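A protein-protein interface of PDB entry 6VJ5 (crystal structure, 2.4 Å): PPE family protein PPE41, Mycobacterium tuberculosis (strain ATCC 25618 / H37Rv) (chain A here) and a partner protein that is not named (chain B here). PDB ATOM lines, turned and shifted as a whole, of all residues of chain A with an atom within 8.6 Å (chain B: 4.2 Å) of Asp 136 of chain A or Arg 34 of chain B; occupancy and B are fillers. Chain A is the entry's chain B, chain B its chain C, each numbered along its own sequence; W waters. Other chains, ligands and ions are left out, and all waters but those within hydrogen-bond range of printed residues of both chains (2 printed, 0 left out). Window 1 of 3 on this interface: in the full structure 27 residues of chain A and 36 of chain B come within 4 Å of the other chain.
OD2 of Asp 136 of chain A lies within salt-bridge range of NH2 of Arg 34 of chain B (3.7 Å).
NH1 of Arg 109 of chain B lies within salt-bridge range of OD1 of Asp 140 of chain A (3.2 Å).
The guanidinium group (NH2) of Arg 116 of chain A lies close to the guanidinium group (NH2) of Arg 34 of chain B (3.2 Å).
The guanidinium group of Arg 113 of chain A is in salt-bridge range of the side-chain carboxylate of Asp 136 of chain A, 3.4 Å away.
The guanidinium group (NE) of Arg 116 of chain A is in salt-bridge range of the side-chain carboxylate (OD1) of Asp 136 of chain A (2.6 Å).
The side-chain carboxylate of Asp 141 of chain A is in hydrogen-bond range of the side-chain amide nitrogen of Gln 137 of chain A (3.4 Å).
O of Gly 97 of chain B lies within hydrogen-bond range of NH1 of Arg 34 of chain B (2.9 Å).
The guanidinium group of Arg 34 of chain B lies within hydrogen-bond range of the backbone carbonyl oxygen of Asp 110 of chain B, 3.0 Å away.
O of Arg 34 of chain B is in hydrogen-bond range of NH1 of Arg 132 of chain B, 2.9 Å away.
Among the printed residues, merely in contact across the chains: Ala 133 of chain A with Glu 32 of chain B (3.1 Å), Gln 137 of chain A with Pro 31 of chain B (3.3 Å), Trp 143 of chain A with Arg 109 of chain B (3.6 Å) and Ala 133 of chain A with Pro 31 of chain B (3.7 Å).
Of chain B, only Arg 34 (3.7 Å) comes within 4 Å of Asp 136 of chain A.
Arg 34 of chain B touches two residues of chain A.
No residue of chain A comes within 4 Å of Cys 35 of chain B.
Printed residues of chain A within 4 Å of Glu 32 of chain B: Ala 133.
Printed residues of chain A within 4 Å of Arg 109 of chain B: Asp 140 and Trp 143.
Asp 141 of chain A touches none of the printed residues of chain B.
Leu 119 of chain A touches none of the printed residues of chain B.
The nearest printed residue of chain B that does not touch Asp 136 of chain A is Pro 31 of chain B (4.3 Å).
The nearest printed residue of chain A that does not touch Pro 31 of chain B is Asp 136 of chain A (4.3 Å).
Along chain A the printed residues that touch a printed residue of chain B span positions 116 to 143.
Of the 13 printed residues of chain B, 4 touch a printed residue of chain A.
Among the printed residues, 7 pairs touch across the chains.
Water W1 lies within hydrogen-bond range of OD2 of Asp 136 of chain A (2.7 Å), NE of Arg 34 of chain B (3.1 Å), O of Pro 31 of chain B (3.2 Å) and NH1 of Arg 117 of chain B (3.3 Å).
Water W2 lies within hydrogen-bond range of the guanidinium group (NH2) of Arg 117 of chain B (2.9 Å), the side-chain carboxylate (OD2) of Asp 136 of chain A (3.3 Å) and the guanidinium group (NH2) of Arg 116 of chain A (3.5 Å).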
ATOM      1  N   ASN A 112      19.828  26.676  10.692  1.00  0.00           N
ATOM      2  CA  ASN A 112      20.678  25.659  10.077  1.00  0.00           C
ATOM      3  C   ASN A 112      20.112  24.261  10.325  1.00  0.00           C
ATOM      4  O   ASN A 112      19.878  23.496   9.386  1.00  0.00           O
ATOM      5  CB  ASN A 112      22.109  25.789  10.618  1.00  0.00           C
ATOM      6  CG  ASN A 112      23.037  24.704  10.108  1.00  0.00           C
ATOM      7  OD1 ASN A 112      23.052  23.598  10.640  1.00  0.00           O
ATOM      8  ND2 ASN A 112      23.842  25.025   9.101  1.00  0.00           N
ATOM      9  N   ARG A 113      19.868  23.918  11.592  1.00  0.00           N
ATOM     10  CA  ARG A 113      19.355  22.588  11.904  1.00  0.00           C
ATOM     11  C   ARG A 113      18.016  22.340  11.222  1.00  0.00           C
ATOM     12  O   ARG A 113      17.768  21.248  10.703  1.00  0.00           O
ATOM     13  CB  ARG A 113      19.213  22.426  13.415  1.00  0.00           C
ATOM     14  CG  ARG A 113      20.505  22.605  14.186  1.00  0.00           C
ATOM     15  CD  ARG A 113      21.477  21.472  13.928  1.00  0.00           C
ATOM     16  NE  ARG A 113      22.213  21.647  12.678  1.00  0.00           N
ATOM     17  CZ  ARG A 113      23.129  20.798  12.230  1.00  0.00           C
ATOM     18  NH1 ARG A 113      23.420  19.712  12.931  1.00  0.00           N
ATOM     19  NH2 ARG A 113      23.755  21.040  11.089  1.00  0.00           N
ATOM     20  N   ARG A 116      18.453  21.680   7.593  1.00  0.00           N
ATOM     21  CA  ARG A 116      19.040  20.361   7.413  1.00  0.00           C
ATOM     22  C   ARG A 116      17.976  19.277   7.466  1.00  0.00           C
ATOM     23  O   ARG A 116      17.998  18.343   6.658  1.00  0.00           O
ATOM     24  CB  ARG A 116      20.108  20.122   8.475  1.00  0.00           C
ATOM     25  CG  ARG A 116      20.913  18.859   8.279  1.00  0.00           C
ATOM     26  CD  ARG A 116      21.609  18.458   9.576  1.00  0.00           C
ATOM     27  NE  ARG A 116      22.748  17.589   9.316  1.00  0.00           N
ATOM     28  CZ  ARG A 116      22.655  16.279   9.119  1.00  0.00           C
ATOM     29  NH1 ARG A 116      21.471  15.677   9.155  1.00  0.00           N
ATOM     30  NH2 ARG A 116      23.751  15.571   8.884  1.00  0.00           N
ATOM     31  N   GLN A 117      17.026  19.387   8.396  1.00  0.00           N
ATOM     32  CA  GLN A 117      16.005  18.355   8.510  1.00  0.00           C
ATOM     33  C   GLN A 117      15.028  18.401   7.341  1.00  0.00           C
ATOM     34  O   GLN A 117      14.431  17.376   6.996  1.00  0.00           O
ATOM     35  CB  GLN A 117      15.245  18.497   9.829  1.00  0.00           C
ATOM     36  CG  GLN A 117      14.452  17.251  10.223  1.00  0.00           C
ATOM     37  CD  GLN A 117      15.343  16.039  10.463  1.00  0.00           C
ATOM     38  OE1 GLN A 117      16.205  16.049  11.345  1.00  0.00           O
ATOM     39  NE2 GLN A 117      15.142  14.992   9.669  1.00  0.00           N
ATOM     40  N   LEU A 119      15.904  19.084   4.229  1.00  0.00           N
ATOM     41  CA  LEU A 119      16.580  18.345   3.171  1.00  0.00           C
ATOM     42  C   LEU A 119      16.558  16.849   3.455  1.00  0.00           C
ATOM     43  O   LEU A 119      16.362  16.041   2.540  1.00  0.00           O
ATOM     44  CB  LEU A 119      18.014  18.839   3.017  1.00  0.00           C
ATOM     45  CG  LEU A 119      18.212  20.301   2.629  1.00  0.00           C
ATOM     46  CD1 LEU A 119      19.717  20.558   2.414  1.00  0.00           C
ATOM     47  CD2 LEU A 119      17.409  20.703   1.415  1.00  0.00           C
ATOM     48  N   ILE A 120      16.753  16.457   4.718  1.00  0.00           N
ATOM     49  CA  ILE A 120      16.674  15.044   5.075  1.00  0.00           C
ATOM     50  C   ILE A 120      15.301  14.494   4.714  1.00  0.00           C
ATOM     51  O   ILE A 120      15.180  13.464   4.038  1.00  0.00           O
ATOM     52  CB  ILE A 120      16.980  14.848   6.571  1.00  0.00           C
ATOM     53  CG1 ILE A 120      18.405  15.303   6.877  1.00  0.00           C
ATOM     54  CG2 ILE A 120      16.780  13.393   6.974  1.00  0.00           C
ATOM     55  CD1 ILE A 120      19.451  14.309   6.462  1.00  0.00           C
ATOM     56  N   THR A 129      22.097  15.303  -0.670  1.00  0.00           N
ATOM     57  CA  THR A 129      23.109  14.861   0.284  1.00  0.00           C
ATOM     58  C   THR A 129      24.235  15.879   0.413  1.00  0.00           C
ATOM     59  O   THR A 129      24.666  16.208   1.522  1.00  0.00           O
ATOM     60  CB  THR A 129      23.661  13.499  -0.136  1.00  0.00           C
ATOM     61  OG1 THR A 129      22.575  12.581  -0.309  1.00  0.00           O
ATOM     62  CG2 THR A 129      24.618  12.958   0.915  1.00  0.00           C
ATOM     63  N   ALA A 130      24.724  16.399  -0.715  1.00  0.00           N
ATOM     64  CA  ALA A 130      25.849  17.330  -0.652  1.00  0.00           C
ATOM     65  C   ALA A 130      25.460  18.623   0.055  1.00  0.00           C
ATOM     66  O   ALA A 130      26.229  19.143   0.872  1.00  0.00           O
ATOM     67  CB  ALA A 130      26.376  17.619  -2.056  1.00  0.00           C
ATOM     68  N   GLN A 131      24.272  19.156  -0.245  1.00  0.00           N
ATOM     69  CA  GLN A 131      23.797  20.350   0.447  1.00  0.00           C
ATOM     70  C   GLN A 131      23.610  20.092   1.936  1.00  0.00           C
ATOM     71  O   GLN A 131      23.695  21.023   2.744  1.00  0.00           O
ATOM     72  CB  GLN A 131      22.486  20.826  -0.179  1.00  0.00           C
ATOM     73  CG  GLN A 131      22.639  21.235  -1.632  1.00  0.00           C
ATOM     74  CD  GLN A 131      21.319  21.566  -2.311  1.00  0.00           C
ATOM     75  OE1 GLN A 131      20.343  21.948  -1.664  1.00  0.00           O
ATOM     76  NE2 GLN A 131      21.286  21.417  -3.627  1.00  0.00           N
ATOM     77  N   ILE A 132      23.337  18.846   2.321  1.00  0.00           N
ATOM     78  CA  ILE A 132      23.284  18.522   3.741  1.00  0.00           C
ATOM     79  C   ILE A 132      24.665  18.667   4.357  1.00  0.00           C
ATOM     80  O   ILE A 132      24.825  19.264   5.427  1.00  0.00           O
ATOM     81  CB  ILE A 132      22.705  17.111   3.937  1.00  0.00           C
ATOM     82  CG1 ILE A 132      21.212  17.121   3.589  1.00  0.00           C
ATOM     83  CG2 ILE A 132      22.945  16.634   5.357  1.00  0.00           C
ATOM     84  CD1 ILE A 132      20.620  15.751   3.375  1.00  0.00           C
ATOM     85  N   ALA A 133      25.687  18.165   3.665  1.00  0.00           N
ATOM     86  CA  ALA A 133      27.055  18.280   4.147  1.00  0.00           C
ATOM     87  C   ALA A 133      27.506  19.736   4.209  1.00  0.00           C
ATOM     88  O   ALA A 133      28.268  20.113   5.106  1.00  0.00           O
ATOM     89  CB  ALA A 133      27.980  17.464   3.246  1.00  0.00           C
ATOM     90  N   ASP A 134      27.048  20.572   3.271  1.00  0.00           N
ATOM     91  CA  ASP A 134      27.338  22.000   3.363  1.00  0.00           C
ATOM     92  C   ASP A 134      26.761  22.583   4.650  1.00  0.00           C
ATOM     93  O   ASP A 134      27.428  23.345   5.359  1.00  0.00           O
ATOM     94  CB  ASP A 134      26.779  22.746   2.147  1.00  0.00           C
ATOM     95  CG  ASP A 134      27.668  22.627   0.912  1.00  0.00           C
ATOM     96  OD1 ASP A 134      28.857  22.281   1.054  1.00  0.00           O
ATOM     97  OD2 ASP A 134      27.173  22.884  -0.209  1.00  0.00           O
ATOM     98  N   LEU A 135      25.512  22.234   4.966  1.00  0.00           N
ATOM     99  CA  LEU A 135      24.899  22.721   6.196  1.00  0.00           C
ATOM    100  C   LEU A 135      25.635  22.211   7.426  1.00  0.00           C
ATOM    101  O   LEU A 135      25.665  22.888   8.458  1.00  0.00           O
ATOM    102  CB  LEU A 135      23.435  22.299   6.252  1.00  0.00           C
ATOM    103  CG  LEU A 135      22.499  23.114   5.361  1.00  0.00           C
ATOM    104  CD1 LEU A 135      21.120  22.486   5.324  1.00  0.00           C
ATOM    105  CD2 LEU A 135      22.423  24.551   5.858  1.00  0.00           C
ATOM    106  N   ASP A 136      26.217  21.018   7.349  1.00  0.00           N
ATOM    107  CA  ASP A 136      27.013  20.536   8.472  1.00  0.00           C
ATOM    108  C   ASP A 136      28.295  21.346   8.620  1.00  0.00           C
ATOM    109  O   ASP A 136      28.755  21.584   9.744  1.00  0.00           O
ATOM    110  CB  ASP A 136      27.327  19.051   8.301  1.00  0.00           C
ATOM    111  CG  ASP A 136      26.150  18.161   8.666  1.00  0.00           C
ATOM    112  OD1 ASP A 136      25.114  18.685   9.130  1.00  0.00           O
ATOM    113  OD2 ASP A 136      26.265  16.933   8.490  1.00  0.00           O
ATOM    114  N   GLN A 137      28.873  21.790   7.501  1.00  0.00           N
ATOM    115  CA  GLN A 137      30.071  22.617   7.578  1.00  0.00           C
ATOM    116  C   GLN A 137      29.754  23.987   8.167  1.00  0.00           C
ATOM    117  O   GLN A 137      30.534  24.522   8.965  1.00  0.00           O
ATOM    118  CB  GLN A 137      30.702  22.768   6.196  1.00  0.00           C
ATOM    119  CG  GLN A 137      32.045  23.489   6.226  1.00  0.00           C
ATOM    120  CD  GLN A 137      33.117  22.705   6.967  1.00  0.00           C
ATOM    121  OE1 GLN A 137      33.665  21.738   6.444  1.00  0.00           O
ATOM    122  NE2 GLN A 137      33.415  23.121   8.195  1.00  0.00           N
ATOM    123  N   GLU A 138      28.620  24.574   7.778  1.00  0.00           N
ATOM    124  CA  GLU A 138      28.219  25.855   8.350  1.00  0.00           C
ATOM    125  C   GLU A 138      28.029  25.743   9.859  1.00  0.00           C
ATOM    126  O   GLU A 138      28.426  26.639  10.611  1.00  0.00           O
ATOM    127  CB  GLU A 138      26.932  26.353   7.685  1.00  0.00           C
ATOM    128  CG  GLU A 138      26.681  27.844   7.875  1.00  0.00           C
ATOM    129  CD  GLU A 138      25.256  28.264   7.547  1.00  0.00           C
ATOM    130  OE1 GLU A 138      24.349  27.402   7.543  1.00  0.00           O
ATOM    131  OE2 GLU A 138      25.040  29.473   7.309  1.00  0.00           O
ATOM    132  N   TYR A 139      27.411  24.655  10.322  1.00  0.00           N
ATOM    133  CA  TYR A 139      27.252  24.465  11.758  1.00  0.00           C
ATOM    134  C   TYR A 139      28.607  24.358  12.445  1.00  0.00           C
ATOM    135  O   TYR A 139      28.823  24.949  13.509  1.00  0.00           O
ATOM    136  CB  TYR A 139      26.403  23.227  12.024  1.00  0.00           C
ATOM    137  CG  TYR A 139      26.229  22.898  13.485  1.00  0.00           C
ATOM    138  CD1 TYR A 139      25.167  23.414  14.211  1.00  0.00           C
ATOM    139  CD2 TYR A 139      27.121  22.057  14.139  1.00  0.00           C
ATOM    140  CE1 TYR A 139      25.004  23.109  15.550  1.00  0.00           C
ATOM    141  CE2 TYR A 139      26.965  21.749  15.469  1.00  0.00           C
ATOM    142  CZ  TYR A 139      25.905  22.276  16.171  1.00  0.00           C
ATOM    143  OH  TYR A 139      25.747  21.969  17.505  1.00  0.00           O
ATOM    144  N   ASP A 140      29.539  23.617  11.843  1.00  0.00           N
ATOM    145  CA  ASP A 140      30.894  23.576  12.378  1.00  0.00           C
ATOM    146  C   ASP A 140      31.546  24.952  12.343  1.00  0.00           C
ATOM    147  O   ASP A 140      32.357  25.268  13.219  1.00  0.00           O
ATOM    148  CB  ASP A 140      31.738  22.572  11.597  1.00  0.00           C
ATOM    149  CG  ASP A 140      31.366  21.129  11.898  1.00  0.00           C
ATOM    150  OD1 ASP A 140      30.649  20.880  12.893  1.00  0.00           O
ATOM    151  OD2 ASP A 140      31.800  20.240  11.134  1.00  0.00           O
ATOM    152  N   ASP A 141      31.229  25.770  11.329  1.00  0.00           N
ATOM    153  CA  ASP A 141      31.732  27.142  11.295  1.00  0.00           C
ATOM    154  C   ASP A 141      31.192  27.946  12.476  1.00  0.00           C
ATOM    155  O   ASP A 141      31.941  28.691  13.118  1.00  0.00           O
ATOM    156  CB  ASP A 141      31.358  27.829   9.973  1.00  0.00           C
ATOM    157  CG  ASP A 141      32.100  27.258   8.751  1.00  0.00           C
ATOM    158  OD1 ASP A 141      33.065  26.470   8.900  1.00  0.00           O
ATOM    159  OD2 ASP A 141      31.711  27.617   7.619  1.00  0.00           O
ATOM    160  N   PHE A 142      29.893  27.815  12.770  1.00  0.00           N
ATOM    161  CA  PHE A 142      29.326  28.428  13.967  1.00  0.00           C
ATOM    162  C   PHE A 142      30.068  27.963  15.219  1.00  0.00           C
ATOM    163  O   PHE A 142      30.411  28.768  16.091  1.00  0.00           O
ATOM    164  CB  PHE A 142      27.839  28.079  14.086  1.00  0.00           C
ATOM    165  CG  PHE A 142      26.973  28.633  12.984  1.00  0.00           C
ATOM    166  CD1 PHE A 142      27.360  29.749  12.262  1.00  0.00           C
ATOM    167  CD2 PHE A 142      25.761  28.030  12.674  1.00  0.00           C
ATOM    168  CE1 PHE A 142      26.557  30.259  11.254  1.00  0.00           C
ATOM    169  CE2 PHE A 142      24.948  28.534  11.659  1.00  0.00           C
ATOM    170  CZ  PHE A 142      25.348  29.650  10.953  1.00  0.00           C
ATOM    171  N   TRP A 143      30.287  26.650  15.338  1.00  0.00           N
ATOM    172  CA  TRP A 143      31.036  26.092  16.462  1.00  0.00           C
ATOM    173  C   TRP A 143      32.391  26.765  16.606  1.00  0.00           C
ATOM    174  O   TRP A 143      32.801  27.145  17.708  1.00  0.00           O
ATOM    175  CB  TRP A 143      31.197  24.585  16.239  1.00  0.00           C
ATOM    176  CG  TRP A 143      31.730  23.778  17.372  1.00  0.00           C
ATOM    177  CD1 TRP A 143      32.713  24.124  18.236  1.00  0.00           C
ATOM    178  CD2 TRP A 143      31.299  22.469  17.754  1.00  0.00           C
ATOM    179  NE1 TRP A 143      32.934  23.111  19.135  1.00  0.00           N
ATOM    180  CE2 TRP A 143      32.071  22.084  18.863  1.00  0.00           C
ATOM    181  CE3 TRP A 143      30.334  21.587  17.266  1.00  0.00           C
ATOM    182  CZ2 TRP A 143      31.907  20.858  19.496  1.00  0.00           C
ATOM    183  CZ3 TRP A 143      30.171  20.371  17.893  1.00  0.00           C
ATOM    184  CH2 TRP A 143      30.954  20.016  18.995  1.00  0.00           C
ATOM    185  N   ALA B  30      37.047  17.318   6.267  1.00  0.00           N
ATOM    186  CA  ALA B  30      35.734  17.093   5.688  1.00  0.00           C
ATOM    187  C   ALA B  30      34.680  17.048   6.795  1.00  0.00           C
ATOM    188  O   ALA B  30      34.887  16.365   7.810  1.00  0.00           O
ATOM    189  CB  ALA B  30      35.715  15.789   4.893  1.00  0.00           C
ATOM    190  N   PRO B  31      33.562  17.758   6.649  1.00  0.00           N
ATOM    191  CA  PRO B  31      32.504  17.665   7.670  1.00  0.00           C
ATOM    192  C   PRO B  31      31.956  16.260   7.840  1.00  0.00           C
ATOM    193  O   PRO B  31      31.447  15.935   8.920  1.00  0.00           O
ATOM    194  CB  PRO B  31      31.426  18.633   7.157  1.00  0.00           C
ATOM    195  CG  PRO B  31      31.680  18.752   5.677  1.00  0.00           C
ATOM    196  CD  PRO B  31      33.166  18.589   5.494  1.00  0.00           C
ATOM    197  N   GLU B  32      32.050  15.409   6.814  1.00  0.00           N
ATOM    198  CA  GLU B  32      31.456  14.078   6.905  1.00  0.00           C
ATOM    199  C   GLU B  32      32.140  13.214   7.956  1.00  0.00           C
ATOM    200  O   GLU B  32      31.519  12.291   8.494  1.00  0.00           O
ATOM    201  CB  GLU B  32      31.510  13.380   5.547  1.00  0.00           C
ATOM    202  CG  GLU B  32      30.586  13.975   4.500  1.00  0.00           C
ATOM    203  CD  GLU B  32      31.184  15.172   3.805  1.00  0.00           C
ATOM    204  OE1 GLU B  32      32.302  15.569   4.180  1.00  0.00           O
ATOM    205  OE2 GLU B  32      30.537  15.711   2.883  1.00  0.00           O
ATOM    206  N   LEU B  33      33.412  13.477   8.253  1.00  0.00           N
ATOM    207  CA  LEU B  33      34.079  12.782   9.346  1.00  0.00           C
ATOM    208  C   LEU B  33      33.587  13.243  10.708  1.00  0.00           C
ATOM    209  O   LEU B  33      33.875  12.579  11.712  1.00  0.00           O
ATOM    210  CB  LEU B  33      35.585  12.990   9.244  1.00  0.00           C
ATOM    211  CG  LEU B  33      36.228  12.368   8.005  1.00  0.00           C
ATOM    212  CD1 LEU B  33      37.550  13.033   7.707  1.00  0.00           C
ATOM    213  CD2 LEU B  33      36.404  10.876   8.231  1.00  0.00           C
ATOM    214  N   ARG B  34      32.875  14.370  10.756  1.00  0.00           N
ATOM    215  CA  ARG B  34      32.208  14.843  11.963  1.00  0.00           C
ATOM    216  C   ARG B  34      33.146  14.814  13.167  1.00  0.00           C
ATOM    217  O   ARG B  34      32.835  14.253  14.221  1.00  0.00           O
ATOM    218  CB  ARG B  34      30.944  14.025  12.221  1.00  0.00           C
ATOM    219  CG  ARG B  34      29.975  14.656  13.193  1.00  0.00           C
ATOM    220  CD  ARG B  34      28.652  13.909  13.201  1.00  0.00           C
ATOM    221  NE  ARG B  34      27.759  14.314  12.117  1.00  0.00           N
ATOM    222  CZ  ARG B  34      26.500  13.900  12.003  1.00  0.00           C
ATOM    223  NH1 ARG B  34      26.001  13.070  12.906  1.00  0.00           N
ATOM    224  NH2 ARG B  34      25.744  14.307  10.993  1.00  0.00           N
ATOM    225  N   CYS B  35      34.304  15.443  13.013  1.00  0.00           N
ATOM    226  CA  CYS B  35      35.216  15.600  14.135  1.00  0.00           C
ATOM    227  C   CYS B  35      34.978  16.932  14.831  1.00  0.00           C
ATOM    228  O   CYS B  35      34.306  17.825  14.309  1.00  0.00           O
ATOM    229  CB  CYS B  35      36.661  15.504  13.662  1.00  0.00           C
ATOM    230  SG  CYS B  35      37.079  13.878  13.023  1.00  0.00           S
ATOM    231  N   GLY B  97      23.441  10.679   8.754  1.00  0.00           N
ATOM    232  CA  GLY B  97      24.037  11.192   9.965  1.00  0.00           C
ATOM    233  C   GLY B  97      23.105  11.335  11.144  1.00  0.00           C
ATOM    234  O   GLY B  97      23.588  11.537  12.269  1.00  0.00           O
ATOM    235  N   SER B 108      26.387  16.674  18.914  1.00  0.00           N
ATOM    236  CA  SER B 108      26.987  15.360  19.083  1.00  0.00           C
ATOM    237  C   SER B 108      27.856  15.021  17.879  1.00  0.00           C
ATOM    238  O   SER B 108      27.486  15.274  16.733  1.00  0.00           O
ATOM    239  CB  SER B 108      25.896  14.303  19.257  1.00  0.00           C
ATOM    240  OG  SER B 108      26.463  13.022  19.460  1.00  0.00           O
ATOM    241  N   ARG B 109      29.025  14.459  18.144  1.00  0.00           N
ATOM    242  CA  ARG B 109      29.891  13.994  17.070  1.00  0.00           C
ATOM    243  C   ARG B 109      29.628  12.535  16.718  1.00  0.00           C
ATOM    244  O   ARG B 109      30.301  11.995  15.834  1.00  0.00           O
ATOM    245  CB  ARG B 109      31.356  14.202  17.458  1.00  0.00           C
ATOM    246  CG  ARG B 109      31.683  15.635  17.912  1.00  0.00           C
ATOM    247  CD  ARG B 109      31.810  16.602  16.737  1.00  0.00           C
ATOM    248  NE  ARG B 109      30.532  17.152  16.286  1.00  0.00           N
ATOM    249  CZ  ARG B 109      30.391  17.905  15.198  1.00  0.00           C
ATOM    250  NH1 ARG B 109      31.449  18.192  14.451  1.00  0.00           N
ATOM    251  NH2 ARG B 109      29.195  18.367  14.849  1.00  0.00           N
ATOM    252  N   ASP B 110      28.661  11.890  17.373  1.00  0.00           N
ATOM    253  CA  ASP B 110      28.326  10.518  17.030  1.00  0.00           C
ATOM    254  C   ASP B 110      27.758  10.450  15.614  1.00  0.00           C
ATOM    255  O   ASP B 110      27.230  11.429  15.075  1.00  0.00           O
ATOM    256  CB  ASP B 110      27.293   9.933  17.994  1.00  0.00           C
ATOM    257  CG  ASP B 110      27.838   9.712  19.387  1.00  0.00           C
ATOM    258  OD1 ASP B 110      29.067   9.536  19.549  1.00  0.00           O
ATOM    259  OD2 ASP B 110      27.012   9.699  20.325  1.00  0.00           O
ATOM    260  N   ILE B 111      27.858   9.269  15.024  1.00  0.00           N
ATOM    261  CA  ILE B 111      27.174   8.959  13.769  1.00  0.00           C
ATOM    262  C   ILE B 111      26.329   7.722  14.005  1.00  0.00           C
ATOM    263  O   ILE B 111      26.548   6.973  14.975  1.00  0.00           O
ATOM    264  CB  ILE B 111      28.172   8.762  12.604  1.00  0.00           C
ATOM    265  CG1 ILE B 111      29.190   7.668  12.920  1.00  0.00           C
ATOM    266  CG2 ILE B 111      28.893  10.063  12.287  1.00  0.00           C
ATOM    267  CD1 ILE B 111      30.135   7.374  11.765  1.00  0.00           C
ATOM    268  N   ARG B 117      31.440   6.055   6.871  1.00  0.00           N
ATOM    269  CA  ARG B 117      31.701   7.296   6.146  1.00  0.00           C
ATOM    270  C   ARG B 117      33.102   7.269   5.558  1.00  0.00           C
ATOM    271  O   ARG B 117      34.085   7.122   6.291  1.00  0.00           O
ATOM    272  CB  ARG B 117      31.530   8.510   7.062  1.00  0.00           C
ATOM    273  CG  ARG B 117      30.109   9.066   7.087  1.00  0.00           C
ATOM    274  CD  ARG B 117      29.681   9.533   8.480  1.00  0.00           C
ATOM    275  NE  ARG B 117      28.316  10.051   8.451  1.00  0.00           N
ATOM    276  CZ  ARG B 117      27.994  11.336   8.314  1.00  0.00           C
ATOM    277  NH1 ARG B 117      28.939  12.262   8.209  1.00  0.00           N
ATOM    278  NH2 ARG B 117      26.719  11.694   8.288  1.00  0.00           N
ATOM    279  N   ARG B 132      35.454   6.662   8.533  1.00  0.00           N
ATOM    280  CA  ARG B 132      34.967   6.669   9.903  1.00  0.00           C
ATOM    281  C   ARG B 132      33.898   5.602  10.094  1.00  0.00           C
ATOM    282  O   ARG B 132      32.951   5.512   9.303  1.00  0.00           O
ATOM    283  CB  ARG B 132      34.403   8.033  10.305  1.00  0.00           C
ATOM    284  CG  ARG B 132      33.737   7.962  11.668  1.00  0.00           C
ATOM    285  CD  ARG B 132      33.451   9.305  12.302  1.00  0.00           C
ATOM    286  NE  ARG B 132      32.821   9.101  13.606  1.00  0.00           N
ATOM    287  CZ  ARG B 132      32.385  10.073  14.396  1.00  0.00           C
ATOM    288  NH1 ARG B 132      32.511  11.341  14.030  1.00  0.00           N
ATOM    289  NH2 ARG B 132      31.820   9.774  15.558  1.00  0.00           N
HETATM  290  O   HOH W   1      28.274  15.331   9.251  1.00  0.00           O
HETATM  291  O   HOH W   2      26.133  14.158   6.788  1.00  0.00           O
